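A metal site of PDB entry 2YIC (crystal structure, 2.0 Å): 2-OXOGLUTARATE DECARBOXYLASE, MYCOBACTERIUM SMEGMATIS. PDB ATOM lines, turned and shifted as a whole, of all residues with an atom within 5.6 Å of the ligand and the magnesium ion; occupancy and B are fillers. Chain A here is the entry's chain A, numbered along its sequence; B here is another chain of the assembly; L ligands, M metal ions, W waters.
OE1 of Gln 617 of chain B sits close to N4 of the ligand (3.2 Å). His 246 touches the ligand (CA to N2, 3.6 Å). CA of Gly 285 touches O2 of the ligand, 3.5 Å away. NE2 of Gln 292 touches C2 of the ligand (3.9 Å). CA of Gly 322 touches O1 of the ligand (3.4 Å). Phe 323 touches the ligand (N to C11, 3.8 Å). OE1 of Gln 542 of chain B touches C5 of the ligand, at 3.1 Å. Leu 591 of chain B touches the ligand. Phe 621 of chain B touches the ligand. Hydrophobic or aromatic side chains that line the ligand: Leu 247, Ala 287, Ala 288, Phe 323, His 388, Leu 591 of chain B and Phe 621 of chain B.
The side-chain carboxylate (OE2) of Glu 593 of chain B sits at hydrogen-bond distance from the side-chain amide nitrogen (NE2) of Gln 542 of chain B. The side-chain carboxylate (OE1) of Glu 593 of chain B lies within hydrogen-bond range of the side-chain amide nitrogen (NE2) of Gln 292 (3.0 Å). The side-chain amide nitrogen (NE2) of Gln 617 of chain B lies within hydrogen-bond range of the backbone carbonyl oxygen (O) of Gln 542 of chain B, 3.4 Å away. The guanidinium group of Arg 384 is in hydrogen-bond range of a ring nitrogen (ND1) of His 388 (3.4 Å). The side-chain amide nitrogen (NE2) of Gln 617 of chain B sits at hydrogen-bond distance from the side-chain carboxylate (OD2) of Asp 543 of chain B (3.2 Å). The backbone carbonyl oxygen (O) of Leu 591 of chain B sits at hydrogen-bond distance from the side-chain amide nitrogen (NE2) of Gln 292 (3.0 Å). O of Phe 323 sits at hydrogen-bond distance from NH1 of Arg 384 (2.8 Å).
Water W3 lies within hydrogen-bond range of the backbone carbonyl oxygen of Val 317, an oxygen (O7) of the ligand, the side-chain amide nitrogen of Asn 319 and the backbone NH of Asp 286. Water W5 lies within hydrogen-bond range of NE2 of His 180 (2.6 Å), O5 of the ligand (2.7 Å), NH2 of Arg 181 (3.2 Å) and NE2 of His 388 (3.4 Å). Water W1 lies within hydrogen-bond range of ND1 of His 388 (2.9 Å), NH1 of Arg 384 (2.9 Å), N of Phe 323 (2.9 Å) and O5 of the ligand (3.1 Å). Water W4 bridges O2 of the ligand (3.0 Å) and N of Gly 285 (3.4 Å). Water W6 bridges OD2 of Asp 543 of chain B and O of Gly 322.
Within 4 Å of the magnesium ion: Asp 286, Asn 319 and Ile 321.
The magnesium ion is bound by O3 of the ligand (2.0 Å), water W3 (2.1 Å), OD1 of Asp 286 (2.1 Å), OD1 of Asn 319 (2.1 Å), O of Ile 321 (2.2 Å) and O6 of the ligand (2.2 Å). The magnesium ion has six donor atoms within binding distance.
An oxygen (O3) of the ligand sits close to the backbone NH (N) of Asp 286 (3.4 Å). An oxygen (O7) of the ligand is in salt-bridge range of the guanidinium group (NE) of Arg 181 (2.7 Å). OE2 of Glu 593 of chain B sits at hydrogen-bond distance from N1 of the ligand (2.7 Å). The backbone carbonyl oxygen (O) of Ser 245 sits at hydrogen-bond distance from a nitrogen (N3) of the ligand (2.9 Å). The backbone NH (N) of Ala 288 lies within hydrogen-bond range of an oxygen (O2) of the ligand (2.9 Å). An oxygen (O2) of the ligand lies within hydrogen-bond range of the backbone NH of Ala 287, 3.5 Å away. The backbone NH (N) of Leu 247 sits at hydrogen-bond distance from a nitrogen (N2) of the ligand, at 3.2 Å. A ring nitrogen (NE2) of His 388 sits close to a sulfur (S1) of the ligand (3.3 Å).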
ATOM      1  N   HIS A 180     -12.800  31.306 -10.983  1.00  0.00           N
ATOM      2  CA  HIS A 180     -13.958  30.700 -11.668  1.00  0.00           C
ATOM      3  C   HIS A 180     -14.609  29.488 -11.012  1.00  0.00           C
ATOM      4  O   HIS A 180     -15.810  29.252 -11.240  1.00  0.00           O
ATOM      5  CB  HIS A 180     -13.585  30.313 -13.110  1.00  0.00           C
ATOM      6  CG  HIS A 180     -12.362  29.457 -13.192  1.00  0.00           C
ATOM      7  ND1 HIS A 180     -11.087  30.008 -13.042  1.00  0.00           N
ATOM      8  CD2 HIS A 180     -12.238  28.133 -13.421  1.00  0.00           C
ATOM      9  CE1 HIS A 180     -10.244  29.001 -13.205  1.00  0.00           C
ATOM     10  NE2 HIS A 180     -10.880  27.859 -13.456  1.00  0.00           N
ATOM     11  N   ARG A 181     -13.847  28.660 -10.263  1.00  0.00           N
ATOM     12  CA  ARG A 181     -14.441  27.446  -9.678  1.00  0.00           C
ATOM     13  C   ARG A 181     -15.624  27.747  -8.732  1.00  0.00           C
ATOM     14  O   ARG A 181     -15.461  28.435  -7.729  1.00  0.00           O
ATOM     15  CB  ARG A 181     -13.386  26.611  -8.940  1.00  0.00           C
ATOM     16  CG  ARG A 181     -13.878  25.228  -8.585  1.00  0.00           C
ATOM     17  CD  ARG A 181     -12.805  24.334  -7.989  1.00  0.00           C
ATOM     18  NE  ARG A 181     -11.620  24.229  -8.845  1.00  0.00           N
ATOM     19  CZ  ARG A 181     -11.523  23.437  -9.907  1.00  0.00           C
ATOM     20  NH1 ARG A 181     -12.558  22.702 -10.294  1.00  0.00           N
ATOM     21  NH2 ARG A 181     -10.399  23.398 -10.607  1.00  0.00           N
ATOM     22  N   SER A 245      -8.940  36.000 -15.965  1.00  0.00           N
ATOM     23  CA  SER A 245      -8.606  34.611 -15.627  1.00  0.00           C
ATOM     24  C   SER A 245      -7.297  34.573 -14.809  1.00  0.00           C
ATOM     25  O   SER A 245      -7.009  33.536 -14.196  1.00  0.00           O
ATOM     26  CB  SER A 245      -8.485  33.748 -16.866  1.00  0.00           C
ATOM     27  OG  SER A 245      -9.668  33.666 -17.634  1.00  0.00           O
ATOM     28  N   HIS A 246      -6.519  35.692 -14.780  1.00  0.00           N
ATOM     29  CA  HIS A 246      -5.264  35.802 -14.002  1.00  0.00           C
ATOM     30  C   HIS A 246      -5.583  35.609 -12.526  1.00  0.00           C
ATOM     31  O   HIS A 246      -6.174  36.499 -11.903  1.00  0.00           O
ATOM     32  CB  HIS A 246      -4.579  37.163 -14.255  1.00  0.00           C
ATOM     33  CG  HIS A 246      -3.998  37.300 -15.642  1.00  0.00           C
ATOM     34  ND1 HIS A 246      -4.790  37.118 -16.789  1.00  0.00           N
ATOM     35  CD2 HIS A 246      -2.729  37.558 -16.030  1.00  0.00           C
ATOM     36  CE1 HIS A 246      -3.973  37.293 -17.818  1.00  0.00           C
ATOM     37  NE2 HIS A 246      -2.734  37.581 -17.422  1.00  0.00           N
ATOM     38  N   LEU A 247      -5.266  34.422 -12.006  1.00  0.00           N
ATOM     39  CA  LEU A 247      -5.554  34.051 -10.618  1.00  0.00           C
ATOM     40  C   LEU A 247      -4.835  35.004  -9.685  1.00  0.00           C
ATOM     41  O   LEU A 247      -3.663  35.320  -9.909  1.00  0.00           O
ATOM     42  CB  LEU A 247      -5.128  32.591 -10.351  1.00  0.00           C
ATOM     43  CG  LEU A 247      -5.823  31.528 -11.262  1.00  0.00           C
ATOM     44  CD1 LEU A 247      -5.176  30.170 -11.101  1.00  0.00           C
ATOM     45  CD2 LEU A 247      -7.325  31.478 -11.008  1.00  0.00           C
ATOM     46  N   GLY A 285      -7.549  29.537  -4.647  1.00  0.00           N
ATOM     47  CA  GLY A 285      -7.208  28.137  -4.883  1.00  0.00           C
ATOM     48  C   GLY A 285      -5.882  27.936  -4.141  1.00  0.00           C
ATOM     49  O   GLY A 285      -5.150  28.909  -3.945  1.00  0.00           O
ATOM     50  N   ASP A 286      -5.549  26.699  -3.752  1.00  0.00           N
ATOM     51  CA  ASP A 286      -4.321  26.432  -2.984  1.00  0.00           C
ATOM     52  C   ASP A 286      -3.056  26.726  -3.755  1.00  0.00           C
ATOM     53  O   ASP A 286      -2.147  27.290  -3.150  1.00  0.00           O
ATOM     54  CB  ASP A 286      -4.280  24.965  -2.500  1.00  0.00           C
ATOM     55  CG  ASP A 286      -4.593  23.906  -3.562  1.00  0.00           C
ATOM     56  OD1 ASP A 286      -5.700  23.940  -4.133  1.00  0.00           O
ATOM     57  OD2 ASP A 286      -3.766  23.008  -3.754  1.00  0.00           O
ATOM     58  N   ALA A 287      -2.964  26.313  -5.045  1.00  0.00           N
ATOM     59  CA  ALA A 287      -1.717  26.539  -5.782  1.00  0.00           C
ATOM     60  C   ALA A 287      -1.486  28.032  -6.039  1.00  0.00           C
ATOM     61  O   ALA A 287      -0.374  28.507  -5.812  1.00  0.00           O
ATOM     62  CB  ALA A 287      -1.713  25.743  -7.099  1.00  0.00           C
ATOM     63  N   ALA A 288      -2.518  28.772  -6.453  1.00  0.00           N
ATOM     64  CA  ALA A 288      -2.401  30.210  -6.742  1.00  0.00           C
ATOM     65  C   ALA A 288      -2.077  31.043  -5.492  1.00  0.00           C
ATOM     66  O   ALA A 288      -1.287  31.984  -5.584  1.00  0.00           O
ATOM     67  CB  ALA A 288      -3.677  30.705  -7.374  1.00  0.00           C
ATOM     68  N   PHE A 289      -2.701  30.708  -4.330  1.00  0.00           N
ATOM     69  CA  PHE A 289      -2.467  31.434  -3.085  1.00  0.00           C
ATOM     70  C   PHE A 289      -0.998  31.352  -2.663  1.00  0.00           C
ATOM     71  O   PHE A 289      -0.447  32.357  -2.214  1.00  0.00           O
ATOM     72  CB  PHE A 289      -3.387  30.873  -1.971  1.00  0.00           C
ATOM     73  CG  PHE A 289      -3.531  31.792  -0.773  1.00  0.00           C
ATOM     74  CD1 PHE A 289      -4.256  32.978  -0.864  1.00  0.00           C
ATOM     75  CD2 PHE A 289      -2.965  31.464   0.451  1.00  0.00           C
ATOM     76  CE1 PHE A 289      -4.392  33.824   0.238  1.00  0.00           C
ATOM     77  CE2 PHE A 289      -3.109  32.311   1.560  1.00  0.00           C
ATOM     78  CZ  PHE A 289      -3.824  33.473   1.454  1.00  0.00           C
ATOM     79  N   GLN A 292       1.477  33.059  -6.237  1.00  0.00           N
ATOM     80  CA  GLN A 292       1.330  34.417  -6.782  1.00  0.00           C
ATOM     81  C   GLN A 292       1.794  35.478  -5.757  1.00  0.00           C
ATOM     82  O   GLN A 292       1.210  35.624  -4.695  1.00  0.00           O
ATOM     83  CB  GLN A 292      -0.140  34.663  -7.209  1.00  0.00           C
ATOM     84  CG  GLN A 292      -0.533  33.890  -8.504  1.00  0.00           C
ATOM     85  CD  GLN A 292       0.157  34.454  -9.739  1.00  0.00           C
ATOM     86  OE1 GLN A 292       0.029  35.636 -10.052  1.00  0.00           O
ATOM     87  NE2 GLN A 292       0.930  33.631 -10.447  1.00  0.00           N
ATOM     88  N   VAL A 317     -10.013  27.405  -1.249  1.00  0.00           N
ATOM     89  CA  VAL A 317     -10.614  26.147  -1.648  1.00  0.00           C
ATOM     90  C   VAL A 317      -9.434  25.219  -1.930  1.00  0.00           C
ATOM     91  O   VAL A 317      -8.848  25.248  -3.023  1.00  0.00           O
ATOM     92  CB  VAL A 317     -11.564  26.324  -2.833  1.00  0.00           C
ATOM     93  CG1 VAL A 317     -12.151  24.966  -3.276  1.00  0.00           C
ATOM     94  CG2 VAL A 317     -12.663  27.317  -2.496  1.00  0.00           C
ATOM     95  N   ASN A 318      -9.006  24.493  -0.887  1.00  0.00           N
ATOM     96  CA  ASN A 318      -7.813  23.689  -0.990  1.00  0.00           C
ATOM     97  C   ASN A 318      -8.134  22.250  -1.407  1.00  0.00           C
ATOM     98  O   ASN A 318      -8.281  21.379  -0.562  1.00  0.00           O
ATOM     99  CB  ASN A 318      -7.046  23.742   0.340  1.00  0.00           C
ATOM    100  CG  ASN A 318      -5.737  22.998   0.340  1.00  0.00           C
ATOM    101  OD1 ASN A 318      -5.324  22.420  -0.669  1.00  0.00           O
ATOM    102  ND2 ASN A 318      -5.108  22.949   1.496  1.00  0.00           N
ATOM    103  N   ASN A 319      -8.166  22.002  -2.738  1.00  0.00           N
ATOM    104  CA  ASN A 319      -8.468  20.652  -3.271  1.00  0.00           C
ATOM    105  C   ASN A 319      -7.170  19.834  -3.452  1.00  0.00           C
ATOM    106  O   ASN A 319      -7.188  18.776  -4.096  1.00  0.00           O
ATOM    107  CB  ASN A 319      -9.246  20.716  -4.542  1.00  0.00           C
ATOM    108  CG  ASN A 319      -8.704  21.695  -5.565  1.00  0.00           C
ATOM    109  OD1 ASN A 319      -7.516  22.042  -5.570  1.00  0.00           O
ATOM    110  ND2 ASN A 319      -9.574  22.142  -6.456  1.00  0.00           N
ATOM    111  N   GLN A 320      -6.044  20.362  -2.915  1.00  0.00           N
ATOM    112  CA  GLN A 320      -4.726  19.688  -2.804  1.00  0.00           C
ATOM    113  C   GLN A 320      -4.153  19.297  -4.166  1.00  0.00           C
ATOM    114  O   GLN A 320      -3.449  18.295  -4.296  1.00  0.00           O
ATOM    115  CB  GLN A 320      -4.867  18.456  -1.883  1.00  0.00           C
ATOM    116  CG  GLN A 320      -5.713  18.727  -0.587  1.00  0.00           C
ATOM    117  CD  GLN A 320      -5.912  17.479   0.253  1.00  0.00           C
ATOM    118  OE1 GLN A 320      -4.955  16.898   0.743  1.00  0.00           O
ATOM    119  NE2 GLN A 320      -7.146  16.978   0.384  1.00  0.00           N
ATOM    120  N   ILE A 321      -4.453  20.121  -5.181  1.00  0.00           N
ATOM    121  CA  ILE A 321      -3.994  19.956  -6.567  1.00  0.00           C
ATOM    122  C   ILE A 321      -4.088  21.296  -7.280  1.00  0.00           C
ATOM    123  O   ILE A 321      -4.956  22.120  -6.953  1.00  0.00           O
ATOM    124  CB  ILE A 321      -4.818  18.830  -7.303  1.00  0.00           C
ATOM    125  CG1 ILE A 321      -4.125  18.363  -8.598  1.00  0.00           C
ATOM    126  CG2 ILE A 321      -6.319  19.209  -7.485  1.00  0.00           C
ATOM    127  CD1 ILE A 321      -4.747  17.055  -9.247  1.00  0.00           C
ATOM    128  N   GLY A 322      -3.189  21.502  -8.236  1.00  0.00           N
ATOM    129  CA  GLY A 322      -3.177  22.701  -9.053  1.00  0.00           C
ATOM    130  C   GLY A 322      -3.093  22.288 -10.503  1.00  0.00           C
ATOM    131  O   GLY A 322      -1.989  22.133 -11.029  1.00  0.00           O
ATOM    132  N   PHE A 323      -4.269  21.977 -11.099  1.00  0.00           N
ATOM    133  CA  PHE A 323      -4.380  21.439 -12.458  1.00  0.00           C
ATOM    134  C   PHE A 323      -3.781  20.015 -12.418  1.00  0.00           C
ATOM    135  O   PHE A 323      -4.496  19.133 -12.000  1.00  0.00           O
ATOM    136  CB  PHE A 323      -3.764  22.385 -13.531  1.00  0.00           C
ATOM    137  CG  PHE A 323      -4.042  22.143 -14.999  1.00  0.00           C
ATOM    138  CD1 PHE A 323      -4.516  20.920 -15.447  1.00  0.00           C
ATOM    139  CD2 PHE A 323      -3.799  23.134 -15.933  1.00  0.00           C
ATOM    140  CE1 PHE A 323      -4.720  20.691 -16.818  1.00  0.00           C
ATOM    141  CE2 PHE A 323      -3.992  22.907 -17.294  1.00  0.00           C
ATOM    142  CZ  PHE A 323      -4.476  21.694 -17.725  1.00  0.00           C
ATOM    143  N   ARG A 384     -11.042  17.740  -5.782  1.00  0.00           N
ATOM    144  CA  ARG A 384     -11.587  18.092  -7.087  1.00  0.00           C
ATOM    145  C   ARG A 384     -12.058  16.804  -7.704  1.00  0.00           C
ATOM    146  O   ARG A 384     -11.236  15.977  -8.075  1.00  0.00           O
ATOM    147  CB  ARG A 384     -10.496  18.825  -7.919  1.00  0.00           C
ATOM    148  CG  ARG A 384     -10.991  19.411  -9.259  1.00  0.00           C
ATOM    149  CD  ARG A 384      -9.833  19.720 -10.202  1.00  0.00           C
ATOM    150  NE  ARG A 384      -9.272  18.464 -10.687  1.00  0.00           N
ATOM    151  CZ  ARG A 384      -8.035  18.305 -11.155  1.00  0.00           C
ATOM    152  NH1 ARG A 384      -7.199  19.341 -11.213  1.00  0.00           N
ATOM    153  NH2 ARG A 384      -7.611  17.116 -11.530  1.00  0.00           N
ATOM    154  N   HIS A 388      -9.242  18.467 -14.463  1.00  0.00           N
ATOM    155  CA  HIS A 388      -9.195  19.929 -14.545  1.00  0.00           C
ATOM    156  C   HIS A 388     -10.147  20.494 -15.596  1.00  0.00           C
ATOM    157  O   HIS A 388     -10.669  21.596 -15.402  1.00  0.00           O
ATOM    158  CB  HIS A 388      -7.802  20.441 -14.831  1.00  0.00           C
ATOM    159  CG  HIS A 388      -7.605  21.843 -14.334  1.00  0.00           C
ATOM    160  ND1 HIS A 388      -7.693  22.161 -12.974  1.00  0.00           N
ATOM    161  CD2 HIS A 388      -7.370  22.982 -15.030  1.00  0.00           C
ATOM    162  CE1 HIS A 388      -7.497  23.464 -12.896  1.00  0.00           C
ATOM    163  NE2 HIS A 388      -7.292  24.004 -14.106  1.00  0.00           N
ATOM    164  N   GLN B 542       4.103  25.700 -16.003  1.00  0.00           N
ATOM    165  CA  GLN B 542       2.922  25.147 -15.346  1.00  0.00           C
ATOM    166  C   GLN B 542       2.386  23.928 -16.088  1.00  0.00           C
ATOM    167  O   GLN B 542       2.126  23.996 -17.298  1.00  0.00           O
ATOM    168  CB  GLN B 542       1.869  26.232 -15.196  1.00  0.00           C
ATOM    169  CG  GLN B 542       2.228  27.231 -14.085  1.00  0.00           C
ATOM    170  CD  GLN B 542       1.627  28.590 -14.340  1.00  0.00           C
ATOM    171  OE1 GLN B 542       0.604  28.730 -15.037  1.00  0.00           O
ATOM    172  NE2 GLN B 542       2.262  29.643 -13.804  1.00  0.00           N
ATOM    173  N   ASP B 543       2.361  22.774 -15.384  1.00  0.00           N
ATOM    174  CA  ASP B 543       1.883  21.482 -15.898  1.00  0.00           C
ATOM    175  C   ASP B 543       2.663  21.034 -17.154  1.00  0.00           C
ATOM    176  O   ASP B 543       2.148  20.238 -17.953  1.00  0.00           O
ATOM    177  CB  ASP B 543       0.394  21.566 -16.131  1.00  0.00           C
ATOM    178  CG  ASP B 543      -0.295  22.010 -14.844  1.00  0.00           C
ATOM    179  OD1 ASP B 543      -0.334  21.199 -13.889  1.00  0.00           O
ATOM    180  OD2 ASP B 543      -0.638  23.207 -14.739  1.00  0.00           O
ATOM    181  N   LEU B 591       2.869  27.923  -9.267  1.00  0.00           N
ATOM    182  CA  LEU B 591       1.955  28.802  -9.958  1.00  0.00           C
ATOM    183  C   LEU B 591       2.458  30.235  -9.852  1.00  0.00           C
ATOM    184  O   LEU B 591       1.911  31.066  -9.125  1.00  0.00           O
ATOM    185  CB  LEU B 591       0.528  28.655  -9.414  1.00  0.00           C
ATOM    186  CG  LEU B 591      -0.578  28.797 -10.453  1.00  0.00           C
ATOM    187  CD1 LEU B 591      -1.843  28.252  -9.931  1.00  0.00           C
ATOM    188  CD2 LEU B 591      -0.768  30.253 -10.911  1.00  0.00           C
ATOM    189  N   GLU B 593       4.687  33.317 -12.392  1.00  0.00           N
ATOM    190  CA  GLU B 593       5.241  33.712 -13.683  1.00  0.00           C
ATOM    191  C   GLU B 593       6.491  34.525 -13.420  1.00  0.00           C
ATOM    192  O   GLU B 593       7.571  34.186 -13.919  1.00  0.00           O
ATOM    193  CB  GLU B 593       4.194  34.498 -14.546  1.00  0.00           C
ATOM    194  CG  GLU B 593       3.129  33.584 -15.133  1.00  0.00           C
ATOM    195  CD  GLU B 593       1.985  33.214 -14.212  1.00  0.00           C
ATOM    196  OE1 GLU B 593       1.679  33.991 -13.291  1.00  0.00           O
ATOM    197  OE2 GLU B 593       1.375  32.144 -14.434  1.00  0.00           O
ATOM    198  N   GLN B 617       1.437  28.750 -19.326  1.00  0.00           N
ATOM    199  CA  GLN B 617       0.301  27.849 -19.513  1.00  0.00           C
ATOM    200  C   GLN B 617      -0.431  28.257 -20.808  1.00  0.00           C
ATOM    201  O   GLN B 617      -0.777  27.424 -21.664  1.00  0.00           O
ATOM    202  CB  GLN B 617      -0.615  27.899 -18.271  1.00  0.00           C
ATOM    203  CG  GLN B 617      -1.814  26.993 -18.420  1.00  0.00           C
ATOM    204  CD  GLN B 617      -1.894  25.999 -17.303  1.00  0.00           C
ATOM    205  OE1 GLN B 617      -2.704  26.137 -16.428  1.00  0.00           O
ATOM    206  NE2 GLN B 617      -1.113  24.948 -17.368  1.00  0.00           N
ATOM    207  N   PHE B 621      -0.612  34.843 -19.770  1.00  0.00           N
ATOM    208  CA  PHE B 621      -0.185  34.958 -18.382  1.00  0.00           C
ATOM    209  C   PHE B 621       1.219  35.436 -18.238  1.00  0.00           C
ATOM    210  O   PHE B 621       1.602  35.838 -17.132  1.00  0.00           O
ATOM    211  CB  PHE B 621      -0.391  33.612 -17.648  1.00  0.00           C
ATOM    212  CG  PHE B 621      -1.845  33.214 -17.682  1.00  0.00           C
ATOM    213  CD1 PHE B 621      -2.823  34.028 -17.127  1.00  0.00           C
ATOM    214  CD2 PHE B 621      -2.245  32.048 -18.329  1.00  0.00           C
ATOM    215  CE1 PHE B 621      -4.165  33.680 -17.199  1.00  0.00           C
ATOM    216  CE2 PHE B 621      -3.603  31.699 -18.403  1.00  0.00           C
ATOM    217  CZ  PHE B 621      -4.547  32.520 -17.857  1.00  0.00           C
ATOM    218  N   HIS B 661      -7.069  33.724 -22.976  1.00  0.00           N
ATOM    219  CA  HIS B 661      -6.655  32.415 -23.512  1.00  0.00           C
ATOM    220  C   HIS B 661      -6.497  32.551 -25.011  1.00  0.00           C
ATOM    221  O   HIS B 661      -6.831  31.635 -25.777  1.00  0.00           O
ATOM    222  CB  HIS B 661      -7.672  31.338 -23.123  1.00  0.00           C
ATOM    223  CG  HIS B 661      -7.745  31.123 -21.646  1.00  0.00           C
ATOM    224  ND1 HIS B 661      -8.591  31.868 -20.861  1.00  0.00           N
ATOM    225  CD2 HIS B 661      -7.001  30.314 -20.861  1.00  0.00           C
ATOM    226  CE1 HIS B 661      -8.379  31.480 -19.619  1.00  0.00           C
ATOM    227  NE2 HIS B 661      -7.423  30.537 -19.571  1.00  0.00           N
HETATM  228  N1  LIG L   1      -1.350  31.915 -14.144  1.00  0.00           N
HETATM  229  C1  LIG L   1      -2.255  32.818 -13.806  1.00  0.00           C
HETATM  230  C2  LIG L   1      -1.808  34.105 -13.183  1.00  0.00           C
HETATM  231  N2  LIG L   1      -3.567  32.583 -13.945  1.00  0.00           N
HETATM  232  C3  LIG L   1      -4.005  31.431 -14.492  1.00  0.00           C
HETATM  233  N3  LIG L   1      -5.353  31.266 -14.715  1.00  0.00           N
HETATM  234  C4  LIG L   1      -3.071  30.438 -14.862  1.00  0.00           C
HETATM  235  C5  LIG L   1      -1.728  30.739 -14.686  1.00  0.00           C
HETATM  236  C6  LIG L   1      -3.511  29.118 -15.473  1.00  0.00           C
HETATM  237  N4  LIG L   1      -4.217  28.209 -14.532  1.00  0.00           N
HETATM  238  C7  LIG L   1      -5.509  28.058 -14.607  1.00  0.00           C
HETATM  239  S1  LIG L   1      -6.081  26.988 -13.394  1.00  0.00           S
HETATM  240  C8  LIG L   1      -4.454  26.693 -12.840  1.00  0.00           C
HETATM  241  C9  LIG L   1      -3.631  27.478 -13.574  1.00  0.00           C
HETATM  242  C10 LIG L   1      -2.145  27.358 -13.339  1.00  0.00           C
HETATM  243  C11 LIG L   1      -4.179  25.764 -11.669  1.00  0.00           C
HETATM  244  C12 LIG L   1      -4.898  26.441 -10.479  1.00  0.00           C
HETATM  245  O1  LIG L   1      -4.709  25.756  -9.239  1.00  0.00           O
HETATM  246  P1  LIG L   1      -5.431  26.235  -7.904  1.00  0.00           P
HETATM  247  O2  LIG L   1      -4.967  27.625  -7.567  1.00  0.00           O
HETATM  248  O3  LIG L   1      -5.091  25.217  -6.731  1.00  0.00           O
HETATM  249  O4  LIG L   1      -7.028  26.211  -8.227  1.00  0.00           O
HETATM  250  P2  LIG L   1      -7.956  25.060  -8.603  1.00  0.00           P
HETATM  251  O5  LIG L   1      -8.128  24.959 -10.165  1.00  0.00           O
HETATM  252  O6  LIG L   1      -7.386  23.780  -8.039  1.00  0.00           O
HETATM  253  O7  LIG L   1      -9.336  25.361  -7.844  1.00  0.00           O
HETATM  254 MG    MG M   1      -6.266  23.675  -6.148  1.00  0.00          MG
HETATM  255  O   HOH W   1      -7.027  22.043 -10.198  1.00  0.00           O
HETATM  256  O   HOH W   2      -9.495  27.966  -7.546  1.00  0.00           O
HETATM  257  O   HOH W   3      -7.854  24.826  -5.435  1.00  0.00           O
HETATM  258  O   HOH W   4      -7.219  29.505  -8.011  1.00  0.00           O
HETATM  259  O   HOH W   5      -9.418  25.965 -12.322  1.00  0.00           O
HETATM  260  O   HOH W   6      -0.638  24.420 -12.236  1.00  0.00           O
